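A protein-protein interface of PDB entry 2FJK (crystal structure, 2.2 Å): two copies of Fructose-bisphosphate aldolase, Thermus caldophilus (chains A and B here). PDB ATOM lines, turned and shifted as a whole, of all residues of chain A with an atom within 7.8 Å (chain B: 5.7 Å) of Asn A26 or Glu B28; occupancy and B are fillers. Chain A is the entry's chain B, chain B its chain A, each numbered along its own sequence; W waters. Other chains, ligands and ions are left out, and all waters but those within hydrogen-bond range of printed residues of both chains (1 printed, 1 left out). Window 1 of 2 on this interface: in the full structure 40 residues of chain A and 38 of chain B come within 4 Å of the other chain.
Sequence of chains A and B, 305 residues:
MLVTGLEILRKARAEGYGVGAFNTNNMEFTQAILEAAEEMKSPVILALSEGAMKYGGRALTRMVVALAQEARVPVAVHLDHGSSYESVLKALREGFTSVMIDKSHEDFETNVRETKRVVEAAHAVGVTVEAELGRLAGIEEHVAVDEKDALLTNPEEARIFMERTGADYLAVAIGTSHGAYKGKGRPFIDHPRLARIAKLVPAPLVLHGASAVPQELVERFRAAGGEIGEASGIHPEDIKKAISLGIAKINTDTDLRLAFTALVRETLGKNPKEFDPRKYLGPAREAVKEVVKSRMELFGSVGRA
ND2 of Asn B26 lies within hydrogen-bond range of OE2 of Glu A28, 3.2 Å away.
OE2 of Glu B28 is in hydrogen-bond range of ND2 of Asn A26 (3.1 Å).
The side-chain carboxylate of Glu B28 sits at hydrogen-bond distance from the side-chain hydroxyl of Tyr A55, 2.6 Å away.
The side-chain amide nitrogen of Gln B31 is in hydrogen-bond range of the backbone carbonyl oxygen of Gly A56 (3.0 Å).
The guanidinium group of Arg B285 lies within hydrogen-bond range of the backbone carbonyl oxygen of Tyr A55 (3.2 Å).
The backbone NH (N) of Glu B28 lies within hydrogen-bond range of the side-chain amide oxygen (OD1) of Asn B26 (3.4 Å).
OD1 of Asn B26 lies within hydrogen-bond range of N of Phe B29, 3.1 Å away.
The backbone carbonyl oxygen (O) of Asn B26 lies within hydrogen-bond range of the side-chain hydroxyl (OG1) of Thr B30.
The guanidinium group (NH1) of Arg B285 sits at hydrogen-bond distance from the side-chain amide oxygen (OE1) of Gln B31, at 2.8 Å.
The side-chain amide oxygen (OD1) of Asn A26 is in hydrogen-bond range of the backbone NH (N) of Phe A29 (3.1 Å).
The backbone carbonyl oxygen of Asn A26 sits at hydrogen-bond distance from the side-chain hydroxyl of Thr A30.
Among the printed residues, pairs that only touch across the chains: Asn A25 with Met B27 (3.9 Å), Asn A26 with Met B27 (3.3 Å), Asn A26 with Leu B281 (3.6 Å), Met A27 with Asn B26 (3.8 Å), Met A27 with Met B27 (3.3 Å), Phe A29 with Pro B277 (3.6 Å), Tyr A55 with Gln B31 (3.7 Å), Tyr A55 with Leu B281 (3.1 Å), Tyr A55 with Gly B282 (3.7 Å), Ala A59 with Met B27 (3.6 Å), Ala A59 with Gln B31 (3.6 Å), Leu A60 with Met B27 (3.6 Å), Leu A281 with Asn B26 (3.7 Å) and Leu A281 with Leu B281 (3.9 Å).
Of chain A, only Asn A26 (3.1 Å) and Tyr A55 (2.6 Å) come within 4 Å of Glu B28.
Printed residues of chain A within 4 Å of Arg B285: Tyr A55.
Of the printed residues of chain B, Tyr A55 touches Glu B28 (2.6 Å), Gln B31 (3.7 Å), Leu B281 (3.1 Å), Gly B282 (3.7 Å) and Arg B285 (3.2 Å).
Of the printed residues of chain B, Glu A28 touches Asn B26 (3.2 Å).
Of the printed residues of chain B, Gly A56 touches Gln B31 (3.0 Å).
Leu A67 touches none of the printed residues of chain B.
The nearest residue of chain A that does not touch Glu B28 is Glu A28 (4.6 Å).
The nearest printed residue of chain B that does not touch Asn A25 is Glu B28 (5.2 Å).
Of the 13 printed residues of chain B, 8 touch a printed residue of chain A.
Of the 23 printed residues of chain A, 10 touch a printed residue of chain B.
Hydrophobic or aromatic side chains of chain A within 4 Å of the printed part of chain B: Met A27, Phe A29, Tyr A55, Ala A59, Leu A60 and Leu A281.
Asn A26 touches Met B27, and with the chains exchanged Met A27 touches Asn B26.
Asn A26 touches Glu B28, and with the chains exchanged Glu A28 touches Asn B26.
Asn A26 touches Leu B281, and with the chains exchanged Leu A281 touches Asn B26.
Leu B281 touches its own counterpart, Leu A281.
Of the 19 pairs that touch across the chains among the printed residues, 8 have their exchanged pair printed and touching as well.
Water W1 lies within hydrogen-bond range of N of Ala A59 (3.2 Å), NE2 of Gln B31 (3.2 Å) and O of Gly A56 (3.3 Å).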
ATOM      1  N   ASN A  23     -17.992  20.260  -7.556  1.00  0.00           N
ATOM      2  CA  ASN A  23     -16.579  19.934  -7.606  1.00  0.00           C
ATOM      3  C   ASN A  23     -16.162  19.125  -6.399  1.00  0.00           C
ATOM      4  O   ASN A  23     -16.610  19.399  -5.283  1.00  0.00           O
ATOM      5  CB  ASN A  23     -15.735  21.210  -7.669  1.00  0.00           C
ATOM      6  CG  ASN A  23     -15.886  21.928  -8.974  1.00  0.00           C
ATOM      7  OD1 ASN A  23     -16.790  22.740  -9.142  1.00  0.00           O
ATOM      8  ND2 ASN A  23     -15.009  21.619  -9.925  1.00  0.00           N
ATOM      9  N   THR A  24     -15.306  18.135  -6.630  1.00  0.00           N
ATOM     10  CA  THR A  24     -14.789  17.291  -5.553  1.00  0.00           C
ATOM     11  C   THR A  24     -13.299  17.059  -5.762  1.00  0.00           C
ATOM     12  O   THR A  24     -12.847  16.960  -6.898  1.00  0.00           O
ATOM     13  CB  THR A  24     -15.447  15.906  -5.529  1.00  0.00           C
ATOM     14  OG1 THR A  24     -16.847  16.049  -5.289  1.00  0.00           O
ATOM     15  CG2 THR A  24     -14.861  15.075  -4.414  1.00  0.00           C
ATOM     16  N   ASN A  25     -12.554  16.953  -4.659  1.00  0.00           N
ATOM     17  CA  ASN A  25     -11.106  16.731  -4.681  1.00  0.00           C
ATOM     18  C   ASN A  25     -10.708  15.513  -3.820  1.00  0.00           C
ATOM     19  O   ASN A  25      -9.551  15.086  -3.838  1.00  0.00           O
ATOM     20  CB  ASN A  25     -10.378  17.981  -4.169  1.00  0.00           C
ATOM     21  CG  ASN A  25     -10.503  19.165  -5.119  1.00  0.00           C
ATOM     22  OD1 ASN A  25      -9.793  19.261  -6.131  1.00  0.00           O
ATOM     23  ND2 ASN A  25     -11.419  20.069  -4.805  1.00  0.00           N
ATOM     24  N   ASN A  26     -11.650  14.970  -3.048  1.00  0.00           N
ATOM     25  CA  ASN A  26     -11.339  13.803  -2.240  1.00  0.00           C
ATOM     26  C   ASN A  26     -12.555  12.960  -1.880  1.00  0.00           C
ATOM     27  O   ASN A  26     -13.660  13.168  -2.399  1.00  0.00           O
ATOM     28  CB  ASN A  26     -10.574  14.201  -0.969  1.00  0.00           C
ATOM     29  CG  ASN A  26     -11.450  14.891   0.054  1.00  0.00           C
ATOM     30  OD1 ASN A  26     -12.667  15.002  -0.117  1.00  0.00           O
ATOM     31  ND2 ASN A  26     -10.831  15.350   1.135  1.00  0.00           N
ATOM     32  N   MET A  27     -12.329  12.000  -0.991  1.00  0.00           N
ATOM     33  CA  MET A  27     -13.364  11.075  -0.567  1.00  0.00           C
ATOM     34  C   MET A  27     -14.567  11.721   0.129  1.00  0.00           C
ATOM     35  O   MET A  27     -15.703  11.535  -0.305  1.00  0.00           O
ATOM     36  CB  MET A  27     -12.766   9.991   0.348  1.00  0.00           C
ATOM     37  CG  MET A  27     -13.776   8.901   0.731  1.00  0.00           C
ATOM     38  SD  MET A  27     -13.149   7.639   2.095  1.00  0.00           S
ATOM     39  CE  MET A  27     -11.881   6.676   1.022  1.00  0.00           C
ATOM     40  N   GLU A  28     -14.324  12.463   1.203  1.00  0.00           N
ATOM     41  CA  GLU A  28     -15.415  13.100   1.949  1.00  0.00           C
ATOM     42  C   GLU A  28     -16.304  13.994   1.098  1.00  0.00           C
ATOM     43  O   GLU A  28     -17.515  14.025   1.298  1.00  0.00           O
ATOM     44  CB  GLU A  28     -14.875  13.902   3.139  1.00  0.00           C
ATOM     45  CG  GLU A  28     -14.371  13.032   4.292  1.00  0.00           C
ATOM     46  CD  GLU A  28     -12.901  12.683   4.168  1.00  0.00           C
ATOM     47  OE1 GLU A  28     -12.373  12.712   3.033  1.00  0.00           O
ATOM     48  OE2 GLU A  28     -12.279  12.370   5.209  1.00  0.00           O
ATOM     49  N   PHE A  29     -15.727  14.719   0.147  1.00  0.00           N
ATOM     50  CA  PHE A  29     -16.560  15.577  -0.700  1.00  0.00           C
ATOM     51  C   PHE A  29     -17.416  14.725  -1.611  1.00  0.00           C
ATOM     52  O   PHE A  29     -18.600  14.994  -1.797  1.00  0.00           O
ATOM     53  CB  PHE A  29     -15.710  16.516  -1.551  1.00  0.00           C
ATOM     54  CG  PHE A  29     -15.342  17.797  -0.855  1.00  0.00           C
ATOM     55  CD1 PHE A  29     -14.470  17.790   0.225  1.00  0.00           C
ATOM     56  CD2 PHE A  29     -15.887  19.010  -1.273  1.00  0.00           C
ATOM     57  CE1 PHE A  29     -14.142  18.970   0.878  1.00  0.00           C
ATOM     58  CE2 PHE A  29     -15.567  20.192  -0.625  1.00  0.00           C
ATOM     59  CZ  PHE A  29     -14.691  20.173   0.455  1.00  0.00           C
ATOM     60  N   THR A  30     -16.813  13.685  -2.178  1.00  0.00           N
ATOM     61  CA  THR A  30     -17.536  12.812  -3.086  1.00  0.00           C
ATOM     62  C   THR A  30     -18.732  12.171  -2.362  1.00  0.00           C
ATOM     63  O   THR A  30     -19.842  12.137  -2.894  1.00  0.00           O
ATOM     64  CB  THR A  30     -16.584  11.738  -3.673  1.00  0.00           C
ATOM     65  OG1 THR A  30     -15.458  12.389  -4.279  1.00  0.00           O
ATOM     66  CG2 THR A  30     -17.278  10.932  -4.734  1.00  0.00           C
ATOM     67  N   GLN A  31     -18.511  11.701  -1.138  1.00  0.00           N
ATOM     68  CA  GLN A  31     -19.580  11.082  -0.356  1.00  0.00           C
ATOM     69  C   GLN A  31     -20.694  12.078  -0.076  1.00  0.00           C
ATOM     70  O   GLN A  31     -21.868  11.778  -0.289  1.00  0.00           O
ATOM     71  CB  GLN A  31     -19.037  10.556   0.975  1.00  0.00           C
ATOM     72  CG  GLN A  31     -17.949   9.504   0.820  1.00  0.00           C
ATOM     73  CD  GLN A  31     -17.341   9.087   2.136  1.00  0.00           C
ATOM     74  OE1 GLN A  31     -16.787   9.907   2.854  1.00  0.00           O
ATOM     75  NE2 GLN A  31     -17.433   7.797   2.455  1.00  0.00           N
ATOM     76  N   ALA A  32     -20.324  13.261   0.410  1.00  0.00           N
ATOM     77  CA  ALA A  32     -21.309  14.293   0.726  1.00  0.00           C
ATOM     78  C   ALA A  32     -22.192  14.581  -0.480  1.00  0.00           C
ATOM     79  O   ALA A  32     -23.418  14.622  -0.367  1.00  0.00           O
ATOM     80  CB  ALA A  32     -20.609  15.574   1.189  1.00  0.00           C
ATOM     81  N   ILE A  33     -21.569  14.765  -1.643  1.00  0.00           N
ATOM     82  CA  ILE A  33     -22.316  15.059  -2.864  1.00  0.00           C
ATOM     83  C   ILE A  33     -23.219  13.906  -3.323  1.00  0.00           C
ATOM     84  O   ILE A  33     -24.339  14.141  -3.783  1.00  0.00           O
ATOM     85  CB  ILE A  33     -21.375  15.402  -4.020  1.00  0.00           C
ATOM     86  CG1 ILE A  33     -20.558  16.647  -3.674  1.00  0.00           C
ATOM     87  CG2 ILE A  33     -22.181  15.626  -5.296  1.00  0.00           C
ATOM     88  CD1 ILE A  33     -19.384  16.876  -4.608  1.00  0.00           C
ATOM     89  N   LEU A  48     -14.735  17.547 -11.735  1.00  0.00           N
ATOM     90  CA  LEU A  48     -13.337  17.436 -11.368  1.00  0.00           C
ATOM     91  C   LEU A  48     -12.435  18.289 -12.252  1.00  0.00           C
ATOM     92  O   LEU A  48     -12.170  17.942 -13.409  1.00  0.00           O
ATOM     93  CB  LEU A  48     -12.864  15.982 -11.433  1.00  0.00           C
ATOM     94  CG  LEU A  48     -13.257  15.075 -10.262  1.00  0.00           C
ATOM     95  CD1 LEU A  48     -14.707  14.669 -10.406  1.00  0.00           C
ATOM     96  CD2 LEU A  48     -12.357  13.845 -10.214  1.00  0.00           C
ATOM     97  N   ALA A  52      -8.113  19.181  -9.433  1.00  0.00           N
ATOM     98  CA  ALA A  52      -8.620  18.017  -8.703  1.00  0.00           C
ATOM     99  C   ALA A  52      -7.908  16.742  -9.135  1.00  0.00           C
ATOM    100  O   ALA A  52      -7.452  15.955  -8.305  1.00  0.00           O
ATOM    101  CB  ALA A  52     -10.132  17.876  -8.923  1.00  0.00           C
ATOM    102  N   TYR A  55      -4.408  16.761  -7.544  1.00  0.00           N
ATOM    103  CA  TYR A  55      -4.454  16.466  -6.110  1.00  0.00           C
ATOM    104  C   TYR A  55      -4.987  15.061  -5.874  1.00  0.00           C
ATOM    105  O   TYR A  55      -4.494  14.333  -5.017  1.00  0.00           O
ATOM    106  CB  TYR A  55      -5.374  17.463  -5.415  1.00  0.00           C
ATOM    107  CG  TYR A  55      -5.534  17.269  -3.923  1.00  0.00           C
ATOM    108  CD1 TYR A  55      -4.571  17.740  -3.034  1.00  0.00           C
ATOM    109  CD2 TYR A  55      -6.676  16.667  -3.399  1.00  0.00           C
ATOM    110  CE1 TYR A  55      -4.739  17.629  -1.664  1.00  0.00           C
ATOM    111  CE2 TYR A  55      -6.863  16.549  -2.019  1.00  0.00           C
ATOM    112  CZ  TYR A  55      -5.887  17.037  -1.157  1.00  0.00           C
ATOM    113  OH  TYR A  55      -6.059  16.945   0.204  1.00  0.00           O
ATOM    114  N   GLY A  56      -5.999  14.689  -6.651  1.00  0.00           N
ATOM    115  CA  GLY A  56      -6.615  13.386  -6.504  1.00  0.00           C
ATOM    116  C   GLY A  56      -5.916  12.215  -7.157  1.00  0.00           C
ATOM    117  O   GLY A  56      -5.910  11.115  -6.601  1.00  0.00           O
ATOM    118  N   ALA A  59      -6.443   7.742  -7.301  1.00  0.00           N
ATOM    119  CA  ALA A  59      -7.304   7.513  -6.164  1.00  0.00           C
ATOM    120  C   ALA A  59      -8.649   8.165  -6.407  1.00  0.00           C
ATOM    121  O   ALA A  59      -9.687   7.516  -6.302  1.00  0.00           O
ATOM    122  CB  ALA A  59      -6.667   8.083  -4.906  1.00  0.00           C
ATOM    123  N   LEU A  60      -8.621   9.444  -6.760  1.00  0.00           N
ATOM    124  CA  LEU A  60      -9.841  10.200  -6.999  1.00  0.00           C
ATOM    125  C   LEU A  60     -10.632   9.776  -8.238  1.00  0.00           C
ATOM    126  O   LEU A  60     -11.822   9.477  -8.128  1.00  0.00           O
ATOM    127  CB  LEU A  60      -9.526  11.700  -7.092  1.00  0.00           C
ATOM    128  CG  LEU A  60     -10.734  12.610  -7.334  1.00  0.00           C
ATOM    129  CD1 LEU A  60     -11.776  12.407  -6.216  1.00  0.00           C
ATOM    130  CD2 LEU A  60     -10.280  14.062  -7.389  1.00  0.00           C
ATOM    131  N   MET A  63     -12.303   6.222  -8.026  1.00  0.00           N
ATOM    132  CA  MET A  63     -13.330   6.207  -6.985  1.00  0.00           C
ATOM    133  C   MET A  63     -14.600   6.947  -7.409  1.00  0.00           C
ATOM    134  O   MET A  63     -15.716   6.485  -7.157  1.00  0.00           O
ATOM    135  CB  MET A  63     -12.806   6.846  -5.711  1.00  0.00           C
ATOM    136  CG  MET A  63     -13.907   7.119  -4.711  1.00  0.00           C
ATOM    137  SD  MET A  63     -13.278   7.955  -3.114  1.00  0.00           S
ATOM    138  CE  MET A  63     -12.761   6.372  -2.164  1.00  0.00           C
ATOM    139  N   VAL A  64     -14.427   8.097  -8.046  1.00  0.00           N
ATOM    140  CA  VAL A  64     -15.568   8.876  -8.493  1.00  0.00           C
ATOM    141  C   VAL A  64     -16.346   8.086  -9.541  1.00  0.00           C
ATOM    142  O   VAL A  64     -17.568   8.001  -9.479  1.00  0.00           O
ATOM    143  CB  VAL A  64     -15.106  10.246  -9.079  1.00  0.00           C
ATOM    144  CG1 VAL A  64     -16.234  10.888  -9.900  1.00  0.00           C
ATOM    145  CG2 VAL A  64     -14.714  11.168  -7.939  1.00  0.00           C
ATOM    146  N   LEU A  67     -18.070   5.079  -7.616  1.00  0.00           N
ATOM    147  CA  LEU A  67     -19.226   5.468  -6.813  1.00  0.00           C
ATOM    148  C   LEU A  67     -20.355   5.962  -7.720  1.00  0.00           C
ATOM    149  O   LEU A  67     -21.520   5.690  -7.463  1.00  0.00           O
ATOM    150  CB  LEU A  67     -18.831   6.535  -5.781  1.00  0.00           C
ATOM    151  CG  LEU A  67     -17.799   6.050  -4.745  1.00  0.00           C
ATOM    152  CD1 LEU A  67     -17.444   7.176  -3.781  1.00  0.00           C
ATOM    153  CD2 LEU A  67     -18.359   4.839  -3.980  1.00  0.00           C
ATOM    154  N   PHE A 260     -16.986  23.334   4.287  1.00  0.00           N
ATOM    155  CA  PHE A 260     -16.087  22.297   4.772  1.00  0.00           C
ATOM    156  C   PHE A 260     -15.035  22.828   5.751  1.00  0.00           C
ATOM    157  O   PHE A 260     -14.801  22.248   6.809  1.00  0.00           O
ATOM    158  CB  PHE A 260     -15.373  21.630   3.590  1.00  0.00           C
ATOM    159  CG  PHE A 260     -14.718  20.324   3.939  1.00  0.00           C
ATOM    160  CD1 PHE A 260     -15.447  19.142   3.923  1.00  0.00           C
ATOM    161  CD2 PHE A 260     -13.379  20.278   4.302  1.00  0.00           C
ATOM    162  CE1 PHE A 260     -14.857  17.934   4.264  1.00  0.00           C
ATOM    163  CE2 PHE A 260     -12.771  19.071   4.646  1.00  0.00           C
ATOM    164  CZ  PHE A 260     -13.514  17.899   4.627  1.00  0.00           C
ATOM    165  N   LEU A 281     -13.134  16.081  10.075  1.00  0.00           N
ATOM    166  CA  LEU A 281     -13.461  15.981   8.650  1.00  0.00           C
ATOM    167  C   LEU A 281     -14.876  15.442   8.448  1.00  0.00           C
ATOM    168  O   LEU A 281     -15.538  15.773   7.467  1.00  0.00           O
ATOM    169  CB  LEU A 281     -12.456  15.066   7.927  1.00  0.00           C
ATOM    170  CG  LEU A 281     -10.967  15.449   7.990  1.00  0.00           C
ATOM    171  CD1 LEU A 281     -10.156  14.427   7.208  1.00  0.00           C
ATOM    172  CD2 LEU A 281     -10.756  16.857   7.418  1.00  0.00           C
ATOM    173  N   ARG A 285     -17.702  17.071   6.319  1.00  0.00           N
ATOM    174  CA  ARG A 285     -18.362  16.341   5.234  1.00  0.00           C
ATOM    175  C   ARG A 285     -19.882  16.529   5.307  1.00  0.00           C
ATOM    176  O   ARG A 285     -20.539  16.732   4.283  1.00  0.00           O
ATOM    177  CB  ARG A 285     -18.028  14.845   5.313  1.00  0.00           C
ATOM    178  CG  ARG A 285     -18.841  13.961   4.364  1.00  0.00           C
ATOM    179  CD  ARG A 285     -18.415  12.493   4.471  1.00  0.00           C
ATOM    180  NE  ARG A 285     -18.535  11.972   5.835  1.00  0.00           N
ATOM    181  CZ  ARG A 285     -17.958  10.846   6.260  1.00  0.00           C
ATOM    182  NH1 ARG A 285     -17.218  10.107   5.437  1.00  0.00           N
ATOM    183  NH2 ARG A 285     -18.107  10.464   7.517  1.00  0.00           N
ATOM    184  N   ASN B  26      -9.209   7.638   4.875  1.00  0.00           N
ATOM    185  CA  ASN B  26      -9.684   8.326   3.682  1.00  0.00           C
ATOM    186  C   ASN B  26      -8.678   8.268   2.533  1.00  0.00           C
ATOM    187  O   ASN B  26      -7.741   7.451   2.543  1.00  0.00           O
ATOM    188  CB  ASN B  26     -10.060   9.787   4.002  1.00  0.00           C
ATOM    189  CG  ASN B  26      -8.868  10.637   4.407  1.00  0.00           C
ATOM    190  OD1 ASN B  26      -7.727  10.191   4.372  1.00  0.00           O
ATOM    191  ND2 ASN B  26      -9.133  11.875   4.786  1.00  0.00           N
ATOM    192  N   MET B  27      -8.889   9.121   1.535  1.00  0.00           N
ATOM    193  CA  MET B  27      -8.009   9.161   0.375  1.00  0.00           C
ATOM    194  C   MET B  27      -6.596   9.642   0.725  1.00  0.00           C
ATOM    195  O   MET B  27      -5.622   8.948   0.469  1.00  0.00           O
ATOM    196  CB  MET B  27      -8.582  10.079  -0.705  1.00  0.00           C
ATOM    197  CG  MET B  27      -7.842   9.983  -2.042  1.00  0.00           C
ATOM    198  SD  MET B  27      -8.476  11.328  -3.287  1.00  0.00           S
ATOM    199  CE  MET B  27     -10.337  10.801  -3.333  1.00  0.00           C
ATOM    200  N   GLU B  28      -6.496  10.824   1.320  1.00  0.00           N
ATOM    201  CA  GLU B  28      -5.188  11.387   1.674  1.00  0.00           C
ATOM    202  C   GLU B  28      -4.253  10.446   2.431  1.00  0.00           C
ATOM    203  O   GLU B  28      -3.051  10.386   2.137  1.00  0.00           O
ATOM    204  CB  GLU B  28      -5.365  12.686   2.467  1.00  0.00           C
ATOM    205  CG  GLU B  28      -5.762  13.893   1.595  1.00  0.00           C
ATOM    206  CD  GLU B  28      -7.267  14.048   1.405  1.00  0.00           C
ATOM    207  OE1 GLU B  28      -8.012  13.070   1.641  1.00  0.00           O
ATOM    208  OE2 GLU B  28      -7.706  15.153   1.013  1.00  0.00           O
ATOM    209  N   PHE B  29      -4.787   9.715   3.408  1.00  0.00           N
ATOM    210  CA  PHE B  29      -3.950   8.790   4.165  1.00  0.00           C
ATOM    211  C   PHE B  29      -3.534   7.609   3.304  1.00  0.00           C
ATOM    212  O   PHE B  29      -2.402   7.135   3.407  1.00  0.00           O
ATOM    213  CB  PHE B  29      -4.667   8.258   5.404  1.00  0.00           C
ATOM    214  CG  PHE B  29      -4.647   9.193   6.584  1.00  0.00           C
ATOM    215  CD1 PHE B  29      -5.425  10.341   6.600  1.00  0.00           C
ATOM    216  CD2 PHE B  29      -3.859   8.909   7.691  1.00  0.00           C
ATOM    217  CE1 PHE B  29      -5.423  11.189   7.694  1.00  0.00           C
ATOM    218  CE2 PHE B  29      -3.849   9.754   8.795  1.00  0.00           C
ATOM    219  CZ  PHE B  29      -4.632  10.894   8.795  1.00  0.00           C
ATOM    220  N   THR B  30      -4.438   7.137   2.448  1.00  0.00           N
ATOM    221  CA  THR B  30      -4.111   5.992   1.615  1.00  0.00           C
ATOM    222  C   THR B  30      -3.026   6.322   0.603  1.00  0.00           C
ATOM    223  O   THR B  30      -2.147   5.505   0.335  1.00  0.00           O
ATOM    224  CB  THR B  30      -5.322   5.455   0.854  1.00  0.00           C
ATOM    225  OG1 THR B  30      -6.407   5.237   1.761  1.00  0.00           O
ATOM    226  CG2 THR B  30      -4.960   4.131   0.199  1.00  0.00           C
ATOM    227  N   GLN B  31      -3.092   7.524   0.039  1.00  0.00           N
ATOM    228  CA  GLN B  31      -2.102   7.960  -0.938  1.00  0.00           C
ATOM    229  C   GLN B  31      -0.728   8.087  -0.290  1.00  0.00           C
ATOM    230  O   GLN B  31       0.280   7.607  -0.832  1.00  0.00           O
ATOM    231  CB  GLN B  31      -2.493   9.314  -1.519  1.00  0.00           C
ATOM    232  CG  GLN B  31      -3.840   9.320  -2.211  1.00  0.00           C
ATOM    233  CD  GLN B  31      -4.190  10.695  -2.739  1.00  0.00           C
ATOM    234  OE1 GLN B  31      -4.240  11.667  -1.986  1.00  0.00           O
ATOM    235  NE2 GLN B  31      -4.426  10.785  -4.037  1.00  0.00           N
ATOM    236  N   ALA B  32      -0.695   8.756   0.863  1.00  0.00           N
ATOM    237  CA  ALA B  32       0.557   8.966   1.591  1.00  0.00           C
ATOM    238  C   ALA B  32       1.229   7.635   1.915  1.00  0.00           C
ATOM    239  O   ALA B  32       2.428   7.451   1.673  1.00  0.00           O
ATOM    240  CB  ALA B  32       0.298   9.747   2.877  1.00  0.00           C
ATOM    241  N   ILE B  33       0.450   6.708   2.457  1.00  0.00           N
ATOM    242  CA  ILE B  33       0.983   5.410   2.807  1.00  0.00           C
ATOM    243  C   ILE B  33       1.543   4.663   1.603  1.00  0.00           C
ATOM    244  O   ILE B  33       2.681   4.195   1.646  1.00  0.00           O
ATOM    245  CB  ILE B  33      -0.075   4.520   3.465  1.00  0.00           C
ATOM    246  CG1 ILE B  33      -0.610   5.180   4.744  1.00  0.00           C
ATOM    247  CG2 ILE B  33       0.532   3.172   3.788  1.00  0.00           C
ATOM    248  CD1 ILE B  33      -1.800   4.440   5.338  1.00  0.00           C
ATOM    249  N   PHE B 260      -0.719  14.471  10.753  1.00  0.00           N
ATOM    250  CA  PHE B 260      -1.751  15.038   9.883  1.00  0.00           C
ATOM    251  C   PHE B 260      -2.460  16.233  10.535  1.00  0.00           C
ATOM    252  O   PHE B 260      -2.606  17.298   9.927  1.00  0.00           O
ATOM    253  CB  PHE B 260      -2.785  13.960   9.553  1.00  0.00           C
ATOM    254  CG  PHE B 260      -3.692  14.318   8.418  1.00  0.00           C
ATOM    255  CD1 PHE B 260      -3.316  14.056   7.107  1.00  0.00           C
ATOM    256  CD2 PHE B 260      -4.917  14.931   8.659  1.00  0.00           C
ATOM    257  CE1 PHE B 260      -4.149  14.401   6.046  1.00  0.00           C
ATOM    258  CE2 PHE B 260      -5.764  15.284   7.603  1.00  0.00           C
ATOM    259  CZ  PHE B 260      -5.382  15.020   6.295  1.00  0.00           C
ATOM    260  N   PRO B 277      -9.643  23.172   0.804  1.00  0.00           N
ATOM    261  CA  PRO B 277      -9.226  21.975   1.535  1.00  0.00           C
ATOM    262  C   PRO B 277      -7.817  21.440   1.255  1.00  0.00           C
ATOM    263  O   PRO B 277      -7.037  21.199   2.178  1.00  0.00           O
ATOM    264  CB  PRO B 277     -10.306  20.961   1.173  1.00  0.00           C
ATOM    265  CG  PRO B 277     -11.529  21.818   1.062  1.00  0.00           C
ATOM    266  CD  PRO B 277     -11.009  23.011   0.272  1.00  0.00           C
ATOM    267  N   LEU B 281      -5.015  19.913   3.690  1.00  0.00           N
ATOM    268  CA  LEU B 281      -5.009  18.448   3.715  1.00  0.00           C
ATOM    269  C   LEU B 281      -3.812  17.945   2.907  1.00  0.00           C
ATOM    270  O   LEU B 281      -3.306  16.851   3.145  1.00  0.00           O
ATOM    271  CB  LEU B 281      -6.296  17.881   3.115  1.00  0.00           C
ATOM    272  CG  LEU B 281      -7.601  18.237   3.818  1.00  0.00           C
ATOM    273  CD1 LEU B 281      -8.756  17.622   3.040  1.00  0.00           C
ATOM    274  CD2 LEU B 281      -7.583  17.740   5.265  1.00  0.00           C
ATOM    275  N   GLY B 282      -3.383  18.755   1.943  1.00  0.00           N
ATOM    276  CA  GLY B 282      -2.247  18.394   1.111  1.00  0.00           C
ATOM    277  C   GLY B 282      -0.973  18.349   1.936  1.00  0.00           C
ATOM    278  O   GLY B 282      -0.264  17.347   1.942  1.00  0.00           O
ATOM    279  N   ARG B 285      -1.177  15.542   4.396  1.00  0.00           N
ATOM    280  CA  ARG B 285      -0.946  14.240   3.763  1.00  0.00           C
ATOM    281  C   ARG B 285       0.544  14.029   3.548  1.00  0.00           C
ATOM    282  O   ARG B 285       1.049  12.919   3.674  1.00  0.00           O
ATOM    283  CB  ARG B 285      -1.669  14.160   2.413  1.00  0.00           C
ATOM    284  CG  ARG B 285      -1.203  13.022   1.493  1.00  0.00           C
ATOM    285  CD  ARG B 285      -1.853  13.124   0.103  1.00  0.00           C
ATOM    286  NE  ARG B 285      -1.525  14.392  -0.554  1.00  0.00           N
ATOM    287  CZ  ARG B 285      -2.168  14.888  -1.611  1.00  0.00           C
ATOM    288  NH1 ARG B 285      -3.179  14.230  -2.153  1.00  0.00           N
ATOM    289  NH2 ARG B 285      -1.810  16.058  -2.119  1.00  0.00           N
HETATM  290  O   HOH W   1      -3.611   8.744  -6.315  1.00  0.00           O
